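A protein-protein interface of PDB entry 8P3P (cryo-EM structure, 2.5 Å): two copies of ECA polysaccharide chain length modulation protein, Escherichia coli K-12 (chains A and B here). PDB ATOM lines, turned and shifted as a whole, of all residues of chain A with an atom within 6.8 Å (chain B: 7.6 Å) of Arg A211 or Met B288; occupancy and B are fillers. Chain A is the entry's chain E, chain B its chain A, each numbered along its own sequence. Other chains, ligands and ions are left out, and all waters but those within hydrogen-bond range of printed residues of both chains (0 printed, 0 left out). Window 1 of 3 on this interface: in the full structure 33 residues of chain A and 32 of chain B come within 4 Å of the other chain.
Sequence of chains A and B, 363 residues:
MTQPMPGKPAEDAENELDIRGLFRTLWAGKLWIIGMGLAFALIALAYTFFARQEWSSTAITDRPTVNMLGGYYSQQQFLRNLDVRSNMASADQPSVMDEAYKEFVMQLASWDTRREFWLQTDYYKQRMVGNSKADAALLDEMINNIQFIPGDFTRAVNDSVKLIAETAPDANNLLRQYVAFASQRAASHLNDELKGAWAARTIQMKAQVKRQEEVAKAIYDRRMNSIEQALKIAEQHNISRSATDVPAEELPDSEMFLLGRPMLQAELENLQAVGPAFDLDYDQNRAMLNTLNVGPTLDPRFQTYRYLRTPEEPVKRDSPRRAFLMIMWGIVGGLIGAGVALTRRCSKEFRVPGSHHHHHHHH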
ATOM      1  N   GLN A 204      34.984   8.275 -13.517  1.00  0.00           N
ATOM      2  CA  GLN A 204      34.446   7.146 -14.268  1.00  0.00           C
ATOM      3  C   GLN A 204      34.993   5.820 -13.749  1.00  0.00           C
ATOM      4  O   GLN A 204      34.249   4.841 -13.616  1.00  0.00           O
ATOM      5  CB  GLN A 204      34.760   7.314 -15.752  1.00  0.00           C
ATOM      6  CG  GLN A 204      34.279   6.173 -16.622  1.00  0.00           C
ATOM      7  CD  GLN A 204      35.309   5.754 -17.647  1.00  0.00           C
ATOM      8  OE1 GLN A 204      35.507   6.429 -18.656  1.00  0.00           O
ATOM      9  NE2 GLN A 204      35.977   4.635 -17.392  1.00  0.00           N
ATOM     10  N   LYS A 206      36.130   5.159 -10.714  1.00  0.00           N
ATOM     11  CA  LYS A 206      35.532   4.881  -9.413  1.00  0.00           C
ATOM     12  C   LYS A 206      34.133   4.299  -9.569  1.00  0.00           C
ATOM     13  O   LYS A 206      33.775   3.327  -8.889  1.00  0.00           O
ATOM     14  CB  LYS A 206      35.491   6.159  -8.577  1.00  0.00           C
ATOM     15  CG  LYS A 206      35.782   5.951  -7.106  1.00  0.00           C
ATOM     16  CD  LYS A 206      36.090   7.268  -6.421  1.00  0.00           C
ATOM     17  CE  LYS A 206      37.275   7.963  -7.067  1.00  0.00           C
ATOM     18  NZ  LYS A 206      37.837   9.025  -6.189  1.00  0.00           N
ATOM     19  N   ALA A 207      33.333   4.871 -10.473  1.00  0.00           N
ATOM     20  CA  ALA A 207      31.994   4.337 -10.707  1.00  0.00           C
ATOM     21  C   ALA A 207      32.051   2.906 -11.231  1.00  0.00           C
ATOM     22  O   ALA A 207      31.266   2.045 -10.806  1.00  0.00           O
ATOM     23  CB  ALA A 207      31.234   5.235 -11.679  1.00  0.00           C
ATOM     24  N   GLN A 208      32.973   2.634 -12.157  1.00  0.00           N
ATOM     25  CA  GLN A 208      33.094   1.288 -12.710  1.00  0.00           C
ATOM     26  C   GLN A 208      33.493   0.277 -11.639  1.00  0.00           C
ATOM     27  O   GLN A 208      32.962  -0.840 -11.597  1.00  0.00           O
ATOM     28  CB  GLN A 208      34.105   1.287 -13.854  1.00  0.00           C
ATOM     29  CG  GLN A 208      34.241  -0.045 -14.561  1.00  0.00           C
ATOM     30  CD  GLN A 208      35.172   0.031 -15.751  1.00  0.00           C
ATOM     31  OE1 GLN A 208      35.614   1.111 -16.139  1.00  0.00           O
ATOM     32  NE2 GLN A 208      35.476  -1.120 -16.339  1.00  0.00           N
ATOM     33  N   VAL A 209      34.430   0.652 -10.767  1.00  0.00           N
ATOM     34  CA  VAL A 209      34.852  -0.246  -9.695  1.00  0.00           C
ATOM     35  C   VAL A 209      33.695  -0.511  -8.738  1.00  0.00           C
ATOM     36  O   VAL A 209      33.494  -1.644  -8.278  1.00  0.00           O
ATOM     37  CB  VAL A 209      36.079   0.332  -8.967  1.00  0.00           C
ATOM     38  CG1 VAL A 209      36.252  -0.311  -7.603  1.00  0.00           C
ATOM     39  CG2 VAL A 209      37.325   0.139  -9.807  1.00  0.00           C
ATOM     40  N   LYS A 210      32.916   0.529  -8.424  1.00  0.00           N
ATOM     41  CA  LYS A 210      31.753   0.340  -7.563  1.00  0.00           C
ATOM     42  C   LYS A 210      30.755  -0.629  -8.189  1.00  0.00           C
ATOM     43  O   LYS A 210      30.211  -1.506  -7.504  1.00  0.00           O
ATOM     44  CB  LYS A 210      31.089   1.688  -7.283  1.00  0.00           C
ATOM     45  CG  LYS A 210      30.091   1.670  -6.144  1.00  0.00           C
ATOM     46  CD  LYS A 210      30.793   1.591  -4.801  1.00  0.00           C
ATOM     47  CE  LYS A 210      31.816   2.703  -4.646  1.00  0.00           C
ATOM     48  NZ  LYS A 210      32.795   2.405  -3.564  1.00  0.00           N
ATOM     49  N   ARG A 211      30.509  -0.489  -9.493  1.00  0.00           N
ATOM     50  CA  ARG A 211      29.592  -1.401 -10.173  1.00  0.00           C
ATOM     51  C   ARG A 211      30.110  -2.835 -10.148  1.00  0.00           C
ATOM     52  O   ARG A 211      29.336  -3.780  -9.951  1.00  0.00           O
ATOM     53  CB  ARG A 211      29.361  -0.941 -11.611  1.00  0.00           C
ATOM     54  CG  ARG A 211      28.257   0.080 -11.756  1.00  0.00           C
ATOM     55  CD  ARG A 211      27.790   0.191 -13.194  1.00  0.00           C
ATOM     56  NE  ARG A 211      28.849   0.657 -14.079  1.00  0.00           N
ATOM     57  CZ  ARG A 211      29.230   1.922 -14.191  1.00  0.00           C
ATOM     58  NH1 ARG A 211      28.664   2.880 -13.475  1.00  0.00           N
ATOM     59  NH2 ARG A 211      30.201   2.235 -15.043  1.00  0.00           N
ATOM     60  N   GLN A 212      31.415  -3.016 -10.362  1.00  0.00           N
ATOM     61  CA  GLN A 212      31.984  -4.361 -10.321  1.00  0.00           C
ATOM     62  C   GLN A 212      31.832  -4.982  -8.939  1.00  0.00           C
ATOM     63  O   GLN A 212      31.490  -6.167  -8.812  1.00  0.00           O
ATOM     64  CB  GLN A 212      33.455  -4.322 -10.730  1.00  0.00           C
ATOM     65  CG  GLN A 212      33.678  -4.392 -12.226  1.00  0.00           C
ATOM     66  CD  GLN A 212      35.129  -4.208 -12.603  1.00  0.00           C
ATOM     67  OE1 GLN A 212      35.859  -3.458 -11.957  1.00  0.00           O
ATOM     68  NE2 GLN A 212      35.557  -4.891 -13.656  1.00  0.00           N
ATOM     69  N   GLU A 213      32.079  -4.196  -7.889  1.00  0.00           N
ATOM     70  CA  GLU A 213      31.896  -4.697  -6.531  1.00  0.00           C
ATOM     71  C   GLU A 213      30.446  -5.093  -6.284  1.00  0.00           C
ATOM     72  O   GLU A 213      30.172  -6.132  -5.669  1.00  0.00           O
ATOM     73  CB  GLU A 213      32.341  -3.647  -5.518  1.00  0.00           C
ATOM     74  CG  GLU A 213      33.810  -3.719  -5.153  1.00  0.00           C
ATOM     75  CD  GLU A 213      34.337  -2.407  -4.612  1.00  0.00           C
ATOM     76  OE1 GLU A 213      33.538  -1.631  -4.051  1.00  0.00           O
ATOM     77  OE2 GLU A 213      35.552  -2.153  -4.747  1.00  0.00           O
ATOM     78  N   GLU A 214      29.503  -4.274  -6.754  1.00  0.00           N
ATOM     79  CA  GLU A 214      28.089  -4.591  -6.569  1.00  0.00           C
ATOM     80  C   GLU A 214      27.711  -5.885  -7.282  1.00  0.00           C
ATOM     81  O   GLU A 214      26.985  -6.721  -6.727  1.00  0.00           O
ATOM     82  CB  GLU A 214      27.230  -3.429  -7.061  1.00  0.00           C
ATOM     83  CG  GLU A 214      25.783  -3.787  -7.336  1.00  0.00           C
ATOM     84  CD  GLU A 214      24.948  -2.580  -7.704  1.00  0.00           C
ATOM     85  OE1 GLU A 214      25.528  -1.490  -7.894  1.00  0.00           O
ATOM     86  OE2 GLU A 214      23.710  -2.719  -7.803  1.00  0.00           O
ATOM     87  N   VAL A 215      28.199  -6.071  -8.510  1.00  0.00           N
ATOM     88  CA  VAL A 215      27.899  -7.292  -9.256  1.00  0.00           C
ATOM     89  C   VAL A 215      28.464  -8.510  -8.539  1.00  0.00           C
ATOM     90  O   VAL A 215      27.793  -9.547  -8.409  1.00  0.00           O
ATOM     91  CB  VAL A 215      28.439  -7.182 -10.694  1.00  0.00           C
ATOM     92  CG1 VAL A 215      28.550  -8.557 -11.328  1.00  0.00           C
ATOM     93  CG2 VAL A 215      27.550  -6.285 -11.526  1.00  0.00           C
ATOM     94  N   ALA A 216      29.709  -8.409  -8.064  1.00  0.00           N
ATOM     95  CA  ALA A 216      30.317  -9.532  -7.360  1.00  0.00           C
ATOM     96  C   ALA A 216      29.547  -9.866  -6.090  1.00  0.00           C
ATOM     97  O   ALA A 216      29.337 -11.043  -5.775  1.00  0.00           O
ATOM     98  CB  ALA A 216      31.777  -9.223  -7.039  1.00  0.00           C
ATOM     99  N   PHE B  78      29.512   9.372 -19.820  1.00  0.00           N
ATOM    100  CA  PHE B  78      28.897   8.133 -19.360  1.00  0.00           C
ATOM    101  C   PHE B  78      27.908   7.616 -20.390  1.00  0.00           C
ATOM    102  O   PHE B  78      27.985   6.457 -20.818  1.00  0.00           O
ATOM    103  CB  PHE B  78      28.213   8.361 -18.012  1.00  0.00           C
ATOM    104  CG  PHE B  78      27.363   7.212 -17.562  1.00  0.00           C
ATOM    105  CD1 PHE B  78      27.940   6.009 -17.198  1.00  0.00           C
ATOM    106  CD2 PHE B  78      25.988   7.336 -17.499  1.00  0.00           C
ATOM    107  CE1 PHE B  78      27.160   4.950 -16.782  1.00  0.00           C
ATOM    108  CE2 PHE B  78      25.203   6.281 -17.083  1.00  0.00           C
ATOM    109  CZ  PHE B  78      25.790   5.087 -16.725  1.00  0.00           C
ATOM    110  N   ASN B  81      29.529   6.118 -23.332  1.00  0.00           N
ATOM    111  CA  ASN B  81      30.019   4.776 -23.039  1.00  0.00           C
ATOM    112  C   ASN B  81      28.965   3.738 -23.386  1.00  0.00           C
ATOM    113  O   ASN B  81      29.241   2.761 -24.093  1.00  0.00           O
ATOM    114  CB  ASN B  81      30.408   4.670 -21.565  1.00  0.00           C
ATOM    115  CG  ASN B  81      31.750   5.301 -21.271  1.00  0.00           C
ATOM    116  OD1 ASN B  81      32.458   5.727 -22.181  1.00  0.00           O
ATOM    117  ND2 ASN B  81      32.107   5.366 -19.995  1.00  0.00           N
ATOM    118  N   LEU B  82      27.730   3.964 -22.933  1.00  0.00           N
ATOM    119  CA  LEU B  82      26.668   3.010 -23.210  1.00  0.00           C
ATOM    120  C   LEU B  82      26.429   2.887 -24.708  1.00  0.00           C
ATOM    121  O   LEU B  82      26.293   1.775 -25.233  1.00  0.00           O
ATOM    122  CB  LEU B  82      25.396   3.427 -22.476  1.00  0.00           C
ATOM    123  CG  LEU B  82      25.571   3.428 -20.957  1.00  0.00           C
ATOM    124  CD1 LEU B  82      24.247   3.578 -20.244  1.00  0.00           C
ATOM    125  CD2 LEU B  82      26.267   2.158 -20.515  1.00  0.00           C
ATOM    126  N   ARG B  85      28.891   0.524 -25.820  1.00  0.00           N
ATOM    127  CA  ARG B  85      28.696  -0.842 -25.346  1.00  0.00           C
ATOM    128  C   ARG B  85      27.586  -1.545 -26.120  1.00  0.00           C
ATOM    129  O   ARG B  85      27.731  -2.711 -26.503  1.00  0.00           O
ATOM    130  CB  ARG B  85      28.387  -0.838 -23.849  1.00  0.00           C
ATOM    131  CG  ARG B  85      29.545  -0.380 -22.974  1.00  0.00           C
ATOM    132  CD  ARG B  85      30.677  -1.395 -22.959  1.00  0.00           C
ATOM    133  NE  ARG B  85      31.705  -1.098 -23.950  1.00  0.00           N
ATOM    134  CZ  ARG B  85      32.627  -0.155 -23.816  1.00  0.00           C
ATOM    135  NH1 ARG B  85      32.680   0.613 -22.740  1.00  0.00           N
ATOM    136  NH2 ARG B  85      33.522   0.021 -24.784  1.00  0.00           N
ATOM    137  N   TRP B 198      19.141  10.339 -21.248  1.00  0.00           N
ATOM    138  CA  TRP B 198      19.208   9.493 -20.063  1.00  0.00           C
ATOM    139  C   TRP B 198      17.914   8.717 -19.867  1.00  0.00           C
ATOM    140  O   TRP B 198      17.942   7.522 -19.550  1.00  0.00           O
ATOM    141  CB  TRP B 198      19.512  10.355 -18.838  1.00  0.00           C
ATOM    142  CG  TRP B 198      19.984   9.597 -17.643  1.00  0.00           C
ATOM    143  CD1 TRP B 198      19.237   8.806 -16.825  1.00  0.00           C
ATOM    144  CD2 TRP B 198      21.314   9.579 -17.113  1.00  0.00           C
ATOM    145  NE1 TRP B 198      20.018   8.288 -15.824  1.00  0.00           N
ATOM    146  CE2 TRP B 198      21.300   8.749 -15.979  1.00  0.00           C
ATOM    147  CE3 TRP B 198      22.516  10.182 -17.491  1.00  0.00           C
ATOM    148  CZ2 TRP B 198      22.439   8.505 -15.219  1.00  0.00           C
ATOM    149  CZ3 TRP B 198      23.645   9.940 -16.737  1.00  0.00           C
ATOM    150  CH2 TRP B 198      23.599   9.108 -15.613  1.00  0.00           C
ATOM    151  N   ARG B 201      17.740   5.928 -22.487  1.00  0.00           N
ATOM    152  CA  ARG B 201      18.648   4.837 -22.152  1.00  0.00           C
ATOM    153  C   ARG B 201      18.120   4.018 -20.981  1.00  0.00           C
ATOM    154  O   ARG B 201      18.240   2.788 -20.972  1.00  0.00           O
ATOM    155  CB  ARG B 201      20.035   5.392 -21.839  1.00  0.00           C
ATOM    156  CG  ARG B 201      21.068   4.327 -21.548  1.00  0.00           C
ATOM    157  CD  ARG B 201      21.110   3.283 -22.647  1.00  0.00           C
ATOM    158  NE  ARG B 201      21.546   3.848 -23.917  1.00  0.00           N
ATOM    159  CZ  ARG B 201      22.104   3.147 -24.894  1.00  0.00           C
ATOM    160  NH1 ARG B 201      22.310   1.845 -24.779  1.00  0.00           N
ATOM    161  NH2 ARG B 201      22.466   3.767 -26.013  1.00  0.00           N
ATOM    162  N   THR B 202      17.539   4.682 -19.979  1.00  0.00           N
ATOM    163  CA  THR B 202      16.968   3.958 -18.848  1.00  0.00           C
ATOM    164  C   THR B 202      15.817   3.067 -19.292  1.00  0.00           C
ATOM    165  O   THR B 202      15.702   1.919 -18.846  1.00  0.00           O
ATOM    166  CB  THR B 202      16.501   4.942 -17.777  1.00  0.00           C
ATOM    167  OG1 THR B 202      17.607   5.745 -17.352  1.00  0.00           O
ATOM    168  CG2 THR B 202      15.940   4.198 -16.579  1.00  0.00           C
ATOM    169  N   MET B 205      17.292   0.046 -21.102  1.00  0.00           N
ATOM    170  CA  MET B 205      17.914  -0.901 -20.181  1.00  0.00           C
ATOM    171  C   MET B 205      16.868  -1.668 -19.383  1.00  0.00           C
ATOM    172  O   MET B 205      17.030  -2.869 -19.137  1.00  0.00           O
ATOM    173  CB  MET B 205      18.877  -0.171 -19.247  1.00  0.00           C
ATOM    174  CG  MET B 205      19.613  -1.088 -18.283  1.00  0.00           C
ATOM    175  SD  MET B 205      21.128  -1.795 -18.959  1.00  0.00           S
ATOM    176  CE  MET B 205      21.553  -0.592 -20.213  1.00  0.00           C
ATOM    177  N   VAL B 209      16.523  -5.719 -19.429  1.00  0.00           N
ATOM    178  CA  VAL B 209      16.555  -6.518 -18.207  1.00  0.00           C
ATOM    179  C   VAL B 209      15.298  -7.371 -18.098  1.00  0.00           C
ATOM    180  O   VAL B 209      15.356  -8.545 -17.706  1.00  0.00           O
ATOM    181  CB  VAL B 209      16.737  -5.606 -16.979  1.00  0.00           C
ATOM    182  CG1 VAL B 209      16.250  -6.296 -15.718  1.00  0.00           C
ATOM    183  CG2 VAL B 209      18.192  -5.205 -16.836  1.00  0.00           C
ATOM    184  N   TYR B 282      23.386 -10.498 -16.964  1.00  0.00           N
ATOM    185  CA  TYR B 282      22.202 -10.012 -16.265  1.00  0.00           C
ATOM    186  C   TYR B 282      22.579  -9.170 -15.054  1.00  0.00           C
ATOM    187  O   TYR B 282      21.986  -8.112 -14.818  1.00  0.00           O
ATOM    188  CB  TYR B 282      21.321 -11.186 -15.846  1.00  0.00           C
ATOM    189  CG  TYR B 282      20.146 -10.786 -14.987  1.00  0.00           C
ATOM    190  CD1 TYR B 282      19.015 -10.219 -15.550  1.00  0.00           C
ATOM    191  CD2 TYR B 282      20.169 -10.977 -13.613  1.00  0.00           C
ATOM    192  CE1 TYR B 282      17.943  -9.852 -14.771  1.00  0.00           C
ATOM    193  CE2 TYR B 282      19.098 -10.615 -12.827  1.00  0.00           C
ATOM    194  CZ  TYR B 282      17.988 -10.053 -13.412  1.00  0.00           C
ATOM    195  OH  TYR B 282      16.916  -9.689 -12.632  1.00  0.00           O
ATOM    196  N   ASP B 283      23.562  -9.620 -14.274  1.00  0.00           N
ATOM    197  CA  ASP B 283      23.974  -8.864 -13.096  1.00  0.00           C
ATOM    198  C   ASP B 283      24.625  -7.543 -13.484  1.00  0.00           C
ATOM    199  O   ASP B 283      24.402  -6.516 -12.829  1.00  0.00           O
ATOM    200  CB  ASP B 283      24.922  -9.703 -12.243  1.00  0.00           C
ATOM    201  CG  ASP B 283      24.217 -10.846 -11.547  1.00  0.00           C
ATOM    202  OD1 ASP B 283      23.334 -10.576 -10.706  1.00  0.00           O
ATOM    203  OD2 ASP B 283      24.542 -12.014 -11.842  1.00  0.00           O
ATOM    204  N   GLN B 284      25.438  -7.549 -14.542  1.00  0.00           N
ATOM    205  CA  GLN B 284      26.039  -6.304 -15.010  1.00  0.00           C
ATOM    206  C   GLN B 284      24.973  -5.324 -15.483  1.00  0.00           C
ATOM    207  O   GLN B 284      25.041  -4.125 -15.183  1.00  0.00           O
ATOM    208  CB  GLN B 284      27.040  -6.597 -16.125  1.00  0.00           C
ATOM    209  CG  GLN B 284      28.296  -7.301 -15.646  1.00  0.00           C
ATOM    210  CD  GLN B 284      29.193  -7.730 -16.786  1.00  0.00           C
ATOM    211  OE1 GLN B 284      28.763  -7.804 -17.936  1.00  0.00           O
ATOM    212  NE2 GLN B 284      30.450  -8.015 -16.473  1.00  0.00           N
ATOM    213  N   ASN B 285      23.975  -5.820 -16.218  1.00  0.00           N
ATOM    214  CA  ASN B 285      22.878  -4.964 -16.656  1.00  0.00           C
ATOM    215  C   ASN B 285      22.090  -4.433 -15.468  1.00  0.00           C
ATOM    216  O   ASN B 285      21.650  -3.281 -15.475  1.00  0.00           O
ATOM    217  CB  ASN B 285      21.962  -5.731 -17.607  1.00  0.00           C
ATOM    218  CG  ASN B 285      22.541  -5.852 -18.999  1.00  0.00           C
ATOM    219  OD1 ASN B 285      23.581  -5.270 -19.301  1.00  0.00           O
ATOM    220  ND2 ASN B 285      21.870  -6.611 -19.853  1.00  0.00           N
ATOM    221  N   ARG B 286      21.894  -5.262 -14.443  1.00  0.00           N
ATOM    222  CA  ARG B 286      21.182  -4.811 -13.253  1.00  0.00           C
ATOM    223  C   ARG B 286      21.945  -3.702 -12.540  1.00  0.00           C
ATOM    224  O   ARG B 286      21.349  -2.714 -12.095  1.00  0.00           O
ATOM    225  CB  ARG B 286      20.943  -5.990 -12.312  1.00  0.00           C
ATOM    226  CG  ARG B 286      19.680  -5.868 -11.489  1.00  0.00           C
ATOM    227  CD  ARG B 286      18.543  -6.655 -12.104  1.00  0.00           C
ATOM    228  NE  ARG B 286      17.351  -6.627 -11.264  1.00  0.00           N
ATOM    229  CZ  ARG B 286      17.224  -7.280 -10.117  1.00  0.00           C
ATOM    230  NH1 ARG B 286      18.194  -8.047  -9.646  1.00  0.00           N
ATOM    231  NH2 ARG B 286      16.093  -7.165  -9.429  1.00  0.00           N
ATOM    232  N   ALA B 287      23.266  -3.846 -12.420  1.00  0.00           N
ATOM    233  CA  ALA B 287      24.064  -2.795 -11.794  1.00  0.00           C
ATOM    234  C   ALA B 287      24.030  -1.511 -12.613  1.00  0.00           C
ATOM    235  O   ALA B 287      23.920  -0.407 -12.058  1.00  0.00           O
ATOM    236  CB  ALA B 287      25.502  -3.272 -11.603  1.00  0.00           C
ATOM    237  N   MET B 288      24.124  -1.631 -13.939  1.00  0.00           N
ATOM    238  CA  MET B 288      24.069  -0.443 -14.783  1.00  0.00           C
ATOM    239  C   MET B 288      22.708   0.231 -14.694  1.00  0.00           C
ATOM    240  O   MET B 288      22.613   1.462 -14.703  1.00  0.00           O
ATOM    241  CB  MET B 288      24.404  -0.807 -16.227  1.00  0.00           C
ATOM    242  CG  MET B 288      24.709   0.392 -17.099  1.00  0.00           C
ATOM    243  SD  MET B 288      26.225   1.213 -16.576  1.00  0.00           S
ATOM    244  CE  MET B 288      27.432   0.399 -17.616  1.00  0.00           C
ATOM    245  N   LEU B 289      21.639  -0.560 -14.597  1.00  0.00           N
ATOM    246  CA  LEU B 289      20.307   0.003 -14.421  1.00  0.00           C
ATOM    247  C   LEU B 289      20.174   0.688 -13.069  1.00  0.00           C
ATOM    248  O   LEU B 289      19.493   1.712 -12.948  1.00  0.00           O
ATOM    249  CB  LEU B 289      19.254  -1.091 -14.576  1.00  0.00           C
ATOM    250  CG  LEU B 289      17.799  -0.647 -14.452  1.00  0.00           C
ATOM    251  CD1 LEU B 289      17.480   0.382 -15.516  1.00  0.00           C
ATOM    252  CD2 LEU B 289      16.873  -1.841 -14.559  1.00  0.00           C
ATOM    253  N   ASN B 290      20.810   0.131 -12.036  1.00  0.00           N
ATOM    254  CA  ASN B 290      20.813   0.788 -10.734  1.00  0.00           C
ATOM    255  C   ASN B 290      21.502   2.143 -10.808  1.00  0.00           C
ATOM    256  O   ASN B 290      21.028   3.122 -10.223  1.00  0.00           O
ATOM    257  CB  ASN B 290      21.497  -0.101  -9.697  1.00  0.00           C
ATOM    258  CG  ASN B 290      20.525  -1.012  -8.981  1.00  0.00           C
ATOM    259  OD1 ASN B 290      19.310  -0.848  -9.086  1.00  0.00           O
ATOM    260  ND2 ASN B 290      21.055  -1.981  -8.246  1.00  0.00           N
ATOM    261  N   THR B 291      22.627   2.217 -11.521  1.00  0.00           N
ATOM    262  CA  THR B 291      23.304   3.503 -11.673  1.00  0.00           C
ATOM    263  C   THR B 291      22.514   4.459 -12.559  1.00  0.00           C
ATOM    264  O   THR B 291      22.609   5.679 -12.388  1.00  0.00           O
ATOM    265  CB  THR B 291      24.710   3.312 -12.235  1.00  0.00           C
ATOM    266  OG1 THR B 291      24.629   2.777 -13.560  1.00  0.00           O
ATOM    267  CG2 THR B 291      25.508   2.374 -11.352  1.00  0.00           C
ATOM    268  N   LEU B 292      21.748   3.934 -13.514  1.00  0.00           N
ATOM    269  CA  LEU B 292      20.931   4.786 -14.370  1.00  0.00           C
ATOM    270  C   LEU B 292      19.703   5.319 -13.645  1.00  0.00           C
ATOM    271  O   LEU B 292      19.217   6.406 -13.976  1.00  0.00           O
ATOM    272  CB  LEU B 292      20.497   4.017 -15.617  1.00  0.00           C
ATOM    273  CG  LEU B 292      21.458   4.009 -16.804  1.00  0.00           C
ATOM    274  CD1 LEU B 292      21.027   2.972 -17.821  1.00  0.00           C
ATOM    275  CD2 LEU B 292      21.530   5.382 -17.438  1.00  0.00           C
ATOM    276  N   ASN B 293      19.189   4.576 -12.664  1.00  0.00           N
ATOM    277  CA  ASN B 293      17.958   4.972 -11.992  1.00  0.00           C
ATOM    278  C   ASN B 293      18.151   6.158 -11.058  1.00  0.00           C
ATOM    279  O   ASN B 293      17.166   6.809 -10.697  1.00  0.00           O
ATOM    280  CB  ASN B 293      17.384   3.790 -11.212  1.00  0.00           C
ATOM    281  CG  ASN B 293      16.411   2.971 -12.032  1.00  0.00           C
ATOM    282  OD1 ASN B 293      15.869   3.445 -13.028  1.00  0.00           O
ATOM    283  ND2 ASN B 293      16.188   1.730 -11.617  1.00  0.00           N
ATOM    284  N   VAL B 294      19.388   6.452 -10.654  1.00  0.00           N
ATOM    285  CA  VAL B 294      19.607   7.587  -9.763  1.00  0.00           C
ATOM    286  C   VAL B 294      19.367   8.899 -10.501  1.00  0.00           C
ATOM    287  O   VAL B 294      19.073   9.926  -9.878  1.00  0.00           O
ATOM    288  CB  VAL B 294      21.018   7.526  -9.146  1.00  0.00           C
ATOM    289  CG1 VAL B 294      22.074   7.858 -10.184  1.00  0.00           C
ATOM    290  CG2 VAL B 294      21.122   8.457  -7.950  1.00  0.00           C
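Of chain B, only Met B288 (3.7 Å) and Thr B291 (3.6 Å) come within 4 Å of Arg A211. Arg B286 touches none of the printed residues of chain A. Of the printed residues of chain A, Ala B287 touches Glu A214 (3.998 Å) and Val A215 (3.6 Å). Of the printed residues of chain A, Thr B291 touches Arg A211. The nearest residue of chain B that does not touch Arg A211 is Ala B287 (4.1 Å). The nearest residue of chain A that does not touch Met B288 is Glu A214 (6.2 Å). The nearest printed residue of chain A that does not touch Asn B81 is Arg A211 (6.2 Å).
1 position is printed for both chains.
Of the 12 printed residues of chain A, 4 touch a printed residue of chain B. Hydrophobic or aromatic side chains of chain A that line the printed part of chain B: Val A215. Of the 22 printed residues of chain B, 7 touch a printed residue of chain A. Among the printed residues, 8 pairs touch across the chains. Among the printed residues, no Asp or Glu carboxylate lies within 4 Å of a Lys or Arg side-chain nitrogen of the other chain.
Gln A204 touches Asn B81 (OE1 to ND2, 3.8 Å). CG of Arg A211 touches CG2 of Thr B291 (3.6 Å). Glu A214 touches Ala B287. Val A215 touches Asp B283. Val A215 touches Gln B284. Ala B287 touches Val A215 (CB to CG2, 3.6 Å).
The backbone carbonyl oxygen of Met B288 sits at hydrogen-bond distance from the side-chain hydroxyl of Thr B291 (2.7 Å).
The side-chain carboxylate of Glu A214 lies within hydrogen-bond range of the side-chain amide nitrogen of Asn B290, at 2.8 Å. SD of Met B288 is in hydrogen-bond range of NE of Arg A211.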
